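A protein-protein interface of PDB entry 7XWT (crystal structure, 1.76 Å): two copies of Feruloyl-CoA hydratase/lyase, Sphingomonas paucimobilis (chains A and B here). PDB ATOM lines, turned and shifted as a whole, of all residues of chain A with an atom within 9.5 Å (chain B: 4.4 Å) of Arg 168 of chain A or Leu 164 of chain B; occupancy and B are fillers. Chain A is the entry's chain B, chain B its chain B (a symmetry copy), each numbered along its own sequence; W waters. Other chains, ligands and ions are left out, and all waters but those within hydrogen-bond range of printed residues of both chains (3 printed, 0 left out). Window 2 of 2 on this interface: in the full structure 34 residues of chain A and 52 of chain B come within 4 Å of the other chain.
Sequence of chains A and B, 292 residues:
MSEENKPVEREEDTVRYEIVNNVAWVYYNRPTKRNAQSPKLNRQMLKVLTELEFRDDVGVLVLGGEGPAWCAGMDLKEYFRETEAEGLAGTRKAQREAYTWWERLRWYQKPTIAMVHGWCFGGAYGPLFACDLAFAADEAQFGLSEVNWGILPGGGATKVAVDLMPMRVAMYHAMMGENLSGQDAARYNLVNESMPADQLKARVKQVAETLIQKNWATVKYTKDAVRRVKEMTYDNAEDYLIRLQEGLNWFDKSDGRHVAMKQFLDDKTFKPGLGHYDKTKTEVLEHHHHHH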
ATOM      1  N   ALA A 161     -32.050  12.177 -20.246  1.00  0.00           N
ATOM      2  CA  ALA A 161     -30.959  12.599 -21.157  1.00  0.00           C
ATOM      3  C   ALA A 161     -31.089  11.844 -22.483  1.00  0.00           C
ATOM      4  O   ALA A 161     -31.008  12.466 -23.572  1.00  0.00           O
ATOM      5  CB  ALA A 161     -29.608  12.403 -20.513  1.00  0.00           C
ATOM      6  N   VAL A 162     -31.362  10.540 -22.410  1.00  0.00           N
ATOM      7  CA  VAL A 162     -31.489   9.699 -23.618  1.00  0.00           C
ATOM      8  C   VAL A 162     -32.780  10.031 -24.396  1.00  0.00           C
ATOM      9  O   VAL A 162     -32.721   9.959 -25.628  1.00  0.00           O
ATOM     10  CB  VAL A 162     -31.394   8.213 -23.222  1.00  0.00           C
ATOM     11  CG1 VAL A 162     -31.933   7.304 -24.307  1.00  0.00           C
ATOM     12  CG2 VAL A 162     -29.962   7.850 -22.893  1.00  0.00           C
ATOM     13  N   MET A 165     -32.047  14.116 -25.761  1.00  0.00           N
ATOM     14  CA  MET A 165     -30.802  14.512 -26.462  1.00  0.00           C
ATOM     15  C   MET A 165     -30.302  13.368 -27.345  1.00  0.00           C
ATOM     16  O   MET A 165     -30.632  12.169 -27.172  1.00  0.00           O
ATOM     17  CB  MET A 165     -29.754  14.943 -25.431  1.00  0.00           C
ATOM     18  CG  MET A 165     -30.220  16.065 -24.515  1.00  0.00           C
ATOM     19  SD  MET A 165     -28.834  16.958 -23.660  1.00  0.00           S
ATOM     20  CE  MET A 165     -28.328  15.613 -22.602  1.00  0.00           C
ATOM     21  N   PRO A 166     -29.492  13.695 -28.357  1.00  0.00           N
ATOM     22  CA  PRO A 166     -28.822  12.675 -29.171  1.00  0.00           C
ATOM     23  C   PRO A 166     -27.950  11.761 -28.290  1.00  0.00           C
ATOM     24  O   PRO A 166     -27.440  12.195 -27.302  1.00  0.00           O
ATOM     25  CB  PRO A 166     -27.994  13.476 -30.201  1.00  0.00           C
ATOM     26  CG  PRO A 166     -28.600  14.878 -30.166  1.00  0.00           C
ATOM     27  CD  PRO A 166     -29.071  15.054 -28.735  1.00  0.00           C
ATOM     28  N   MET A 167     -27.933  10.459 -28.586  1.00  0.00           N
ATOM     29  CA  MET A 167     -27.205   9.442 -27.798  1.00  0.00           C
ATOM     30  C   MET A 167     -25.788   9.937 -27.483  1.00  0.00           C
ATOM     31  O   MET A 167     -25.373   9.838 -26.333  1.00  0.00           O
ATOM     32  CB  MET A 167     -27.120   8.121 -28.558  1.00  0.00           C
ATOM     33  CG  MET A 167     -26.192   7.150 -27.902  1.00  0.00           C
ATOM     34  SD  MET A 167     -26.362   5.502 -28.572  1.00  0.00           S
ATOM     35  CE  MET A 167     -25.447   4.537 -27.365  1.00  0.00           C
ATOM     36  N   ARG A 168     -25.046  10.423 -28.473  1.00  0.00           N
ATOM     37  CA  ARG A 168     -23.646  10.843 -28.213  1.00  0.00           C
ATOM     38  C   ARG A 168     -23.623  11.881 -27.108  1.00  0.00           C
ATOM     39  O   ARG A 168     -22.738  11.771 -26.195  1.00  0.00           O
ATOM     40  CB  ARG A 168     -22.967  11.448 -29.441  1.00  0.00           C
ATOM     41  CG  ARG A 168     -22.536  10.420 -30.464  1.00  0.00           C
ATOM     42  CD  ARG A 168     -21.455   9.480 -29.967  1.00  0.00           C
ATOM     43  NE  ARG A 168     -20.997   8.675 -31.091  1.00  0.00           N
ATOM     44  CZ  ARG A 168     -20.368   7.511 -30.986  1.00  0.00           C
ATOM     45  NH1 ARG A 168     -20.014   7.042 -29.797  1.00  0.00           N
ATOM     46  NH2 ARG A 168     -20.002   6.901 -32.093  1.00  0.00           N
ATOM     47  N   VAL A 169     -24.540  12.855 -27.195  1.00  0.00           N
ATOM     48  CA  VAL A 169     -24.616  14.004 -26.248  1.00  0.00           C
ATOM     49  C   VAL A 169     -24.999  13.457 -24.884  1.00  0.00           C
ATOM     50  O   VAL A 169     -24.341  13.791 -23.898  1.00  0.00           O
ATOM     51  CB  VAL A 169     -25.562  15.110 -26.740  1.00  0.00           C
ATOM     52  CG1 VAL A 169     -25.691  16.222 -25.713  1.00  0.00           C
ATOM     53  CG2 VAL A 169     -25.092  15.647 -28.089  1.00  0.00           C
ATOM     54  N   ALA A 170     -25.981  12.566 -24.811  1.00  0.00           N
ATOM     55  CA  ALA A 170     -26.385  11.992 -23.514  1.00  0.00           C
ATOM     56  C   ALA A 170     -25.204  11.248 -22.875  1.00  0.00           C
ATOM     57  O   ALA A 170     -25.013  11.335 -21.641  1.00  0.00           O
ATOM     58  CB  ALA A 170     -27.586  11.111 -23.695  1.00  0.00           C
ATOM     59  N   MET A 171     -24.424  10.521 -23.668  1.00  0.00           N
ATOM     60  CA  MET A 171     -23.312   9.673 -23.173  1.00  0.00           C
ATOM     61  C   MET A 171     -22.236  10.582 -22.568  1.00  0.00           C
ATOM     62  O   MET A 171     -21.823  10.384 -21.451  1.00  0.00           O
ATOM     63  CB  MET A 171     -22.736   8.839 -24.330  1.00  0.00           C
ATOM     64  CG  MET A 171     -21.649   7.915 -23.927  1.00  0.00           C
ATOM     65  SD  MET A 171     -22.309   6.534 -22.941  1.00  0.00           S
ATOM     66  CE  MET A 171     -23.114   5.572 -24.208  1.00  0.00           C
ATOM     67  N   TYR A 172     -21.821  11.577 -23.312  1.00  0.00           N
ATOM     68  CA  TYR A 172     -20.817  12.550 -22.843  1.00  0.00           C
ATOM     69  C   TYR A 172     -21.313  13.206 -21.549  1.00  0.00           C
ATOM     70  O   TYR A 172     -20.532  13.308 -20.577  1.00  0.00           O
ATOM     71  CB  TYR A 172     -20.527  13.565 -23.939  1.00  0.00           C
ATOM     72  CG  TYR A 172     -19.396  14.490 -23.596  1.00  0.00           C
ATOM     73  CD1 TYR A 172     -19.599  15.612 -22.801  1.00  0.00           C
ATOM     74  CD2 TYR A 172     -18.098  14.198 -23.992  1.00  0.00           C
ATOM     75  CE1 TYR A 172     -18.550  16.467 -22.492  1.00  0.00           C
ATOM     76  CE2 TYR A 172     -17.039  15.038 -23.675  1.00  0.00           C
ATOM     77  CZ  TYR A 172     -17.267  16.181 -22.926  1.00  0.00           C
ATOM     78  OH  TYR A 172     -16.184  16.970 -22.600  1.00  0.00           O
ATOM     79  N   HIS A 173     -22.584  13.628 -21.525  1.00  0.00           N
ATOM     80  CA  HIS A 173     -23.193  14.381 -20.411  1.00  0.00           C
ATOM     81  C   HIS A 173     -23.151  13.558 -19.124  1.00  0.00           C
ATOM     82  O   HIS A 173     -22.757  14.099 -18.093  1.00  0.00           O
ATOM     83  CB  HIS A 173     -24.605  14.812 -20.805  1.00  0.00           C
ATOM     84  CG  HIS A 173     -25.141  15.969 -20.050  1.00  0.00           C
ATOM     85  ND1 HIS A 173     -26.319  15.873 -19.334  1.00  0.00           N
ATOM     86  CD2 HIS A 173     -24.689  17.245 -19.939  1.00  0.00           C
ATOM     87  CE1 HIS A 173     -26.600  17.064 -18.844  1.00  0.00           C
ATOM     88  NE2 HIS A 173     -25.589  17.912 -19.171  1.00  0.00           N
ATOM     89  N   ALA A 174     -23.527  12.284 -19.198  1.00  0.00           N
ATOM     90  CA  ALA A 174     -23.562  11.393 -18.045  1.00  0.00           C
ATOM     91  C   ALA A 174     -22.156  10.945 -17.599  1.00  0.00           C
ATOM     92  O   ALA A 174     -21.991  10.716 -16.413  1.00  0.00           O
ATOM     93  CB  ALA A 174     -24.388  10.194 -18.398  1.00  0.00           C
ATOM     94  N   MET A 175     -21.222  10.701 -18.518  1.00  0.00           N
ATOM     95  CA  MET A 175     -19.885  10.159 -18.195  1.00  0.00           C
ATOM     96  C   MET A 175     -18.969  11.281 -17.690  1.00  0.00           C
ATOM     97  O   MET A 175     -18.167  11.012 -16.793  1.00  0.00           O
ATOM     98  CB  MET A 175     -19.232   9.494 -19.410  1.00  0.00           C
ATOM     99  CG  MET A 175     -19.918   8.234 -19.895  1.00  0.00           C
ATOM    100  SD  MET A 175     -19.188   7.675 -21.480  1.00  0.00           S
ATOM    101  CE  MET A 175     -17.608   7.100 -20.901  1.00  0.00           C
ATOM    102  N   MET A 176     -19.033  12.471 -18.271  1.00  0.00           N
ATOM    103  CA  MET A 176     -18.009  13.511 -18.029  1.00  0.00           C
ATOM    104  C   MET A 176     -18.447  14.465 -16.907  1.00  0.00           C
ATOM    105  O   MET A 176     -17.574  15.129 -16.328  1.00  0.00           O
ATOM    106  CB  MET A 176     -17.735  14.266 -19.321  1.00  0.00           C
ATOM    107  CG  MET A 176     -17.181  13.382 -20.399  1.00  0.00           C
ATOM    108  SD  MET A 176     -15.447  12.879 -20.147  1.00  0.00           S
ATOM    109  CE  MET A 176     -14.679  14.423 -20.645  1.00  0.00           C
ATOM    110  N   LEU A 180     -23.926  21.872 -19.421  1.00  0.00           N
ATOM    111  CA  LEU A 180     -24.378  22.544 -20.652  1.00  0.00           C
ATOM    112  C   LEU A 180     -24.901  23.905 -20.245  1.00  0.00           C
ATOM    113  O   LEU A 180     -25.652  23.991 -19.247  1.00  0.00           O
ATOM    114  CB  LEU A 180     -25.475  21.730 -21.343  1.00  0.00           C
ATOM    115  CG  LEU A 180     -25.029  20.372 -21.869  1.00  0.00           C
ATOM    116  CD1 LEU A 180     -26.246  19.535 -22.227  1.00  0.00           C
ATOM    117  CD2 LEU A 180     -24.086  20.551 -23.042  1.00  0.00           C
ATOM    118  N   TYR A 188     -29.197  21.069 -28.137  1.00  0.00           N
ATOM    119  CA  TYR A 188     -29.275  19.587 -28.042  1.00  0.00           C
ATOM    120  C   TYR A 188     -30.652  19.144 -27.568  1.00  0.00           C
ATOM    121  O   TYR A 188     -30.799  17.923 -27.301  1.00  0.00           O
ATOM    122  CB  TYR A 188     -28.213  19.035 -27.092  1.00  0.00           C
ATOM    123  CG  TYR A 188     -26.798  19.236 -27.550  1.00  0.00           C
ATOM    124  CD1 TYR A 188     -26.407  18.839 -28.810  1.00  0.00           C
ATOM    125  CD2 TYR A 188     -25.847  19.765 -26.701  1.00  0.00           C
ATOM    126  CE1 TYR A 188     -25.103  19.003 -29.238  1.00  0.00           C
ATOM    127  CE2 TYR A 188     -24.532  19.931 -27.108  1.00  0.00           C
ATOM    128  CZ  TYR A 188     -24.160  19.536 -28.381  1.00  0.00           C
ATOM    129  OH  TYR A 188     -22.875  19.695 -28.827  1.00  0.00           O
ATOM    130  N   LEU B 128     -17.409   2.097 -34.543  1.00  0.00           N
ATOM    131  CA  LEU B 128     -17.668   3.538 -34.231  1.00  0.00           C
ATOM    132  C   LEU B 128     -18.749   3.701 -33.145  1.00  0.00           C
ATOM    133  O   LEU B 128     -18.567   4.477 -32.180  1.00  0.00           O
ATOM    134  CB  LEU B 128     -18.066   4.286 -35.497  1.00  0.00           C
ATOM    135  CG  LEU B 128     -18.380   5.771 -35.298  1.00  0.00           C
ATOM    136  CD1 LEU B 128     -17.185   6.510 -34.745  1.00  0.00           C
ATOM    137  CD2 LEU B 128     -18.867   6.407 -36.573  1.00  0.00           C
ATOM    138  N   PHE B 129     -19.830   2.941 -33.257  1.00  0.00           N
ATOM    139  CA  PHE B 129     -20.957   2.976 -32.307  1.00  0.00           C
ATOM    140  C   PHE B 129     -20.561   2.299 -30.987  1.00  0.00           C
ATOM    141  O   PHE B 129     -21.055   2.686 -29.912  1.00  0.00           O
ATOM    142  CB  PHE B 129     -22.179   2.298 -32.936  1.00  0.00           C
ATOM    143  CG  PHE B 129     -23.392   2.245 -32.035  1.00  0.00           C
ATOM    144  CD1 PHE B 129     -24.324   3.266 -32.051  1.00  0.00           C
ATOM    145  CD2 PHE B 129     -23.671   1.127 -31.268  1.00  0.00           C
ATOM    146  CE1 PHE B 129     -25.452   3.220 -31.254  1.00  0.00           C
ATOM    147  CE2 PHE B 129     -24.802   1.076 -30.471  1.00  0.00           C
ATOM    148  CZ  PHE B 129     -25.706   2.116 -30.472  1.00  0.00           C
ATOM    149  N   CYS B 131     -17.735   2.297 -29.494  1.00  0.00           N
ATOM    150  CA  CYS B 131     -17.078   3.293 -28.668  1.00  0.00           C
ATOM    151  C   CYS B 131     -18.143   4.204 -28.039  1.00  0.00           C
ATOM    152  O   CYS B 131     -19.070   4.653 -28.762  1.00  0.00           O
ATOM    153  CB  CYS B 131     -16.081   4.082 -29.520  1.00  0.00           C
ATOM    154  SG  CYS B 131     -14.665   3.106 -30.102  1.00  0.00           S
ATOM    155  N   ASP B 132     -17.989   4.486 -26.742  1.00  0.00           N
ATOM    156  CA  ASP B 132     -18.929   5.280 -25.934  1.00  0.00           C
ATOM    157  C   ASP B 132     -18.909   6.705 -26.503  1.00  0.00           C
ATOM    158  O   ASP B 132     -19.963   7.299 -26.716  1.00  0.00           O
ATOM    159  CB  ASP B 132     -18.554   5.199 -24.459  1.00  0.00           C
ATOM    160  CG  ASP B 132     -18.513   3.773 -23.952  1.00  0.00           C
ATOM    161  OD1 ASP B 132     -19.324   2.991 -24.464  1.00  0.00           O
ATOM    162  OD2 ASP B 132     -17.632   3.444 -23.108  1.00  0.00           O
ATOM    163  N   LEU B 133     -17.722   7.205 -26.729  1.00  0.00           N
ATOM    164  CA  LEU B 133     -17.540   8.604 -27.194  1.00  0.00           C
ATOM    165  C   LEU B 133     -16.759   8.566 -28.507  1.00  0.00           C
ATOM    166  O   LEU B 133     -16.053   7.561 -28.798  1.00  0.00           O
ATOM    167  CB  LEU B 133     -16.789   9.416 -26.128  1.00  0.00           C
ATOM    168  CG  LEU B 133     -17.384   9.527 -24.716  1.00  0.00           C
ATOM    169  CD1 LEU B 133     -16.442  10.287 -23.778  1.00  0.00           C
ATOM    170  CD2 LEU B 133     -18.756  10.169 -24.742  1.00  0.00           C
ATOM    171  N   ALA B 134     -16.821   9.650 -29.278  1.00  0.00           N
ATOM    172  CA  ALA B 134     -16.184   9.706 -30.603  1.00  0.00           C
ATOM    173  C   ALA B 134     -15.808  11.149 -30.925  1.00  0.00           C
ATOM    174  O   ALA B 134     -16.616  12.101 -30.769  1.00  0.00           O
ATOM    175  CB  ALA B 134     -17.055   9.073 -31.663  1.00  0.00           C
ATOM    176  N   VAL B 160     -26.762   1.598 -36.565  1.00  0.00           N
ATOM    177  CA  VAL B 160     -25.855   2.632 -36.008  1.00  0.00           C
ATOM    178  C   VAL B 160     -26.362   3.985 -36.467  1.00  0.00           C
ATOM    179  O   VAL B 160     -26.463   4.926 -35.617  1.00  0.00           O
ATOM    180  CB  VAL B 160     -24.402   2.391 -36.435  1.00  0.00           C
ATOM    181  CG1 VAL B 160     -23.496   3.593 -36.130  1.00  0.00           C
ATOM    182  CG2 VAL B 160     -23.886   1.143 -35.808  1.00  0.00           C
ATOM    183  N   ALA B 161     -26.590   4.126 -37.765  1.00  0.00           N
ATOM    184  CA  ALA B 161     -27.004   5.412 -38.376  1.00  0.00           C
ATOM    185  C   ALA B 161     -28.336   5.855 -37.765  1.00  0.00           C
ATOM    186  O   ALA B 161     -28.485   7.039 -37.371  1.00  0.00           O
ATOM    187  CB  ALA B 161     -27.070   5.301 -39.880  1.00  0.00           C
ATOM    188  N   VAL B 162     -29.272   4.916 -37.611  1.00  0.00           N
ATOM    189  CA  VAL B 162     -30.605   5.223 -37.053  1.00  0.00           C
ATOM    190  C   VAL B 162     -30.521   5.532 -35.544  1.00  0.00           C
ATOM    191  O   VAL B 162     -31.297   6.389 -35.108  1.00  0.00           O
ATOM    192  CB  VAL B 162     -31.576   4.070 -37.376  1.00  0.00           C
ATOM    193  CG1 VAL B 162     -32.807   4.105 -36.495  1.00  0.00           C
ATOM    194  CG2 VAL B 162     -31.971   4.112 -38.836  1.00  0.00           C
ATOM    195  N   ASP B 163     -29.615   4.911 -34.778  1.00  0.00           N
ATOM    196  CA  ASP B 163     -29.555   5.075 -33.301  1.00  0.00           C
ATOM    197  C   ASP B 163     -28.798   6.364 -32.984  1.00  0.00           C
ATOM    198  O   ASP B 163     -29.105   6.955 -31.979  1.00  0.00           O
ATOM    199  CB  ASP B 163     -29.031   3.830 -32.592  1.00  0.00           C
ATOM    200  CG  ASP B 163     -30.115   2.781 -32.306  1.00  0.00           C
ATOM    201  OD1 ASP B 163     -31.261   2.901 -32.871  1.00  0.00           O
ATOM    202  OD2 ASP B 163     -29.815   1.808 -31.546  1.00  0.00           O
ATOM    203  N   LEU B 164     -27.969   6.875 -33.879  1.00  0.00           N
ATOM    204  CA  LEU B 164     -27.159   8.080 -33.581  1.00  0.00           C
ATOM    205  C   LEU B 164     -27.717   9.346 -34.230  1.00  0.00           C
ATOM    206  O   LEU B 164     -27.519  10.464 -33.643  1.00  0.00           O
ATOM    207  CB  LEU B 164     -25.728   7.851 -34.070  1.00  0.00           C
ATOM    208  CG  LEU B 164     -24.921   6.793 -33.321  1.00  0.00           C
ATOM    209  CD1 LEU B 164     -23.520   6.671 -33.888  1.00  0.00           C
ATOM    210  CD2 LEU B 164     -24.900   7.059 -31.826  1.00  0.00           C
ATOM    211  N   MET B 165     -28.218   9.244 -35.459  1.00  0.00           N
ATOM    212  CA  MET B 165     -28.565  10.419 -36.296  1.00  0.00           C
ATOM    213  C   MET B 165     -30.081  10.528 -36.458  1.00  0.00           C
ATOM    214  O   MET B 165     -30.864   9.560 -36.287  1.00  0.00           O
ATOM    215  CB  MET B 165     -27.848  10.307 -37.645  1.00  0.00           C
ATOM    216  CG  MET B 165     -26.338  10.174 -37.529  1.00  0.00           C
ATOM    217  SD  MET B 165     -25.426  10.586 -39.094  1.00  0.00           S
ATOM    218  CE  MET B 165     -25.989   9.189 -40.049  1.00  0.00           C
ATOM    219  N   TYR B 188     -24.661  16.157 -36.757  1.00  0.00           N
ATOM    220  CA  TYR B 188     -25.765  15.160 -36.800  1.00  0.00           C
ATOM    221  C   TYR B 188     -25.560  14.076 -35.752  1.00  0.00           C
ATOM    222  O   TYR B 188     -26.344  13.091 -35.788  1.00  0.00           O
ATOM    223  CB  TYR B 188     -25.878  14.516 -38.180  1.00  0.00           C
ATOM    224  CG  TYR B 188     -26.274  15.456 -39.280  1.00  0.00           C
ATOM    225  CD1 TYR B 188     -27.393  16.251 -39.154  1.00  0.00           C
ATOM    226  CD2 TYR B 188     -25.565  15.502 -40.463  1.00  0.00           C
ATOM    227  CE1 TYR B 188     -27.777  17.108 -40.166  1.00  0.00           C
ATOM    228  CE2 TYR B 188     -25.938  16.348 -41.494  1.00  0.00           C
ATOM    229  CZ  TYR B 188     -27.059  17.147 -41.345  1.00  0.00           C
ATOM    230  OH  TYR B 188     -27.454  18.008 -42.334  1.00  0.00           O
ATOM    231  N   ASN B 189     -24.557  14.225 -34.874  1.00  0.00           N
ATOM    232  CA  ASN B 189     -24.399  13.424 -33.633  1.00  0.00           C
ATOM    233  C   ASN B 189     -23.953  11.993 -33.971  1.00  0.00           C
ATOM    234  O   ASN B 189     -24.165  11.090 -33.136  1.00  0.00           O
ATOM    235  CB  ASN B 189     -25.702  13.483 -32.814  1.00  0.00           C
ATOM    236  CG  ASN B 189     -26.242  14.900 -32.707  1.00  0.00           C
ATOM    237  OD1 ASN B 189     -27.332  15.191 -33.181  1.00  0.00           O
ATOM    238  ND2 ASN B 189     -25.507  15.795 -32.066  1.00  0.00           N
ATOM    239  N   LEU B 190     -23.282  11.790 -35.110  1.00  0.00           N
ATOM    240  CA  LEU B 190     -22.493  10.557 -35.372  1.00  0.00           C
ATOM    241  C   LEU B 190     -21.300  10.530 -34.404  1.00  0.00           C
ATOM    242  O   LEU B 190     -20.959   9.473 -33.905  1.00  0.00           O
ATOM    243  CB  LEU B 190     -22.069  10.526 -36.841  1.00  0.00           C
ATOM    244  CG  LEU B 190     -21.670   9.161 -37.375  1.00  0.00           C
ATOM    245  CD1 LEU B 190     -22.845   8.211 -37.295  1.00  0.00           C
ATOM    246  CD2 LEU B 190     -21.177   9.292 -38.811  1.00  0.00           C
ATOM    247  N   VAL B 191     -20.707  11.684 -34.133  1.00  0.00           N
ATOM    248  CA  VAL B 191     -19.599  11.818 -33.160  1.00  0.00           C
ATOM    249  C   VAL B 191     -19.941  12.958 -32.195  1.00  0.00           C
ATOM    250  O   VAL B 191     -20.887  13.705 -32.493  1.00  0.00           O
ATOM    251  CB  VAL B 191     -18.280  12.074 -33.897  1.00  0.00           C
ATOM    252  CG1 VAL B 191     -17.990  10.952 -34.893  1.00  0.00           C
ATOM    253  CG2 VAL B 191     -18.315  13.427 -34.577  1.00  0.00           C
ATOM    254  N   ASN B 192     -19.150  13.105 -31.134  1.00  0.00           N
ATOM    255  CA  ASN B 192     -19.323  14.147 -30.108  1.00  0.00           C
ATOM    256  C   ASN B 192     -18.820  15.476 -30.655  1.00  0.00           C
ATOM    257  O   ASN B 192     -19.482  16.496 -30.405  1.00  0.00           O
ATOM    258  CB  ASN B 192     -18.587  13.777 -28.830  1.00  0.00           C
ATOM    259  CG  ASN B 192     -19.258  12.602 -28.153  1.00  0.00           C
ATOM    260  OD1 ASN B 192     -18.901  11.451 -28.378  1.00  0.00           O
ATOM    261  ND2 ASN B 192     -20.236  12.918 -27.339  1.00  0.00           N
HETATM  262  O   HOH W   1     -25.910  10.622 -31.178  1.00  0.00           O
HETATM  263  O   HOH W   2     -29.296   9.512 -30.978  1.00  0.00           O
HETATM  264  O   HOH W   3     -22.034  16.914 -29.257  1.00  0.00           O
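Ala 161 of chain A touches none of the printed residues of chain B. Printed residues of chain B within 4 Å of Arg 168 of chain A: Leu 128, Cys 131, Asp 132, Leu 133, Ala 134, Leu 164, Asn 189, Leu 190 and Asn 192. Printed residues of chain A within 4 Å of Leu 128 of chain B: Arg 168 (2.8 Å). Asp 163 of chain B touches none of the printed residues of chain A. Leu 164 of chain B touches just these residues of chain A: Met 167 and Arg 168. Printed residues of chain A within 4 Å of Leu 190 of chain B: Arg 168 (2.9 Å). The nearest printed residue of chain B that does not touch Arg 168 of chain A is Val 191 of chain B (4.01 Å).
The backbone carbonyl oxygen of Leu 128 of chain B lies within hydrogen-bond range of the guanidinium group of Arg 168 of chain A. The guanidinium group (NH1) of Arg 168 of chain A lies within hydrogen-bond range of the backbone carbonyl oxygen (O) of Cys 131 of chain B (2.8 Å). The backbone carbonyl oxygen (O) of Asp 132 of chain B sits at hydrogen-bond distance from the guanidinium group (NH1) of Arg 168 of chain A (3.1 Å). NE of Arg 168 of chain A is in hydrogen-bond range of O of Leu 190 of chain B, at 2.9 Å. The backbone carbonyl oxygen (O) of Arg 168 of chain A is in hydrogen-bond range of the side-chain amide nitrogen (ND2) of Asn 192 of chain B (3.0 Å).
Printed residues of chain A that touch a printed residue of chain B: Pro 166, Met 167, Arg 168, Met 171, Tyr 172 and Met 175. Hydrophobic or aromatic side chains of chain A that line the printed part of chain B: Pro 166, Met 167, Met 171, Tyr 172 and Met 175. Of the 17 printed residues of chain B, 10 touch a printed residue of chain A. Printed residues of chain B that touch a printed residue of chain A: Leu 128, Phe 129, Cys 131, Asp 132, Leu 133, Ala 134, Leu 164, Asn 189, Leu 190 and Asn 192. Hydrophobic or aromatic side chains of chain B that line the printed part of chain A: Leu 128, Phe 129, Leu 133, Ala 134 and Leu 164. Among the printed residues, 17 pairs touch across the chains.
Water W1 lies within hydrogen-bond range of the backbone carbonyl oxygen (O) of Asn 189 of chain B (2.7 Å), the backbone NH (N) of Arg 168 of chain A (2.8 Å), the backbone carbonyl oxygen (O) of Leu 164 of chain B (2.9 Å) and the backbone NH (N) of Met 167 of chain A (3.3 Å). Water W2 lies within hydrogen-bond range of the backbone carbonyl oxygen (O) of Asp 163 of chain B (2.8 Å), the backbone NH (N) of Met 167 of chain A (2.9 Å) and the backbone carbonyl oxygen (O) of Leu 164 of chain B (3.3 Å). Water W3 bridges O of Asn 192 of chain B (2.8 Å) and OH of Tyr 188 of chain A (2.9 Å).
Among the printed residues, merely in contact across the chains: Arg 168 of chain A with Asn 189 of chain B (3.2 Å), Pro 166 of chain A with Asn 189 of chain B (3.3 Å), Met 171 of chain A with Asp 132 of chain B (3.3 Å), Tyr 172 of chain A with Asn 192 of chain B (3.5 Å), Met 167 of chain A with Phe 129 of chain B (3.6 Å), Tyr 172 of chain A with Leu 133 of chain B (3.7 Å), Arg 168 of chain A with Ala 134 of chain B (3.7 Å), Met 171 of chain A with Leu 133 of chain B (3.8 Å), Arg 168 of chain A with Leu 133 of chain B (3.8 Å), Met 167 of chain A with Leu 164 of chain B (3.9 Å), Met 175 of chain A with Asp 132 of chain B (3.9 Å) and Arg 168 of chain A with Leu 164 of chain B (3.96 Å).
4 positions are printed for both chains.
O of Ala 134 of chain B is in hydrogen-bond range of N of Asn 192 of chain B, at 2.7 Å.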
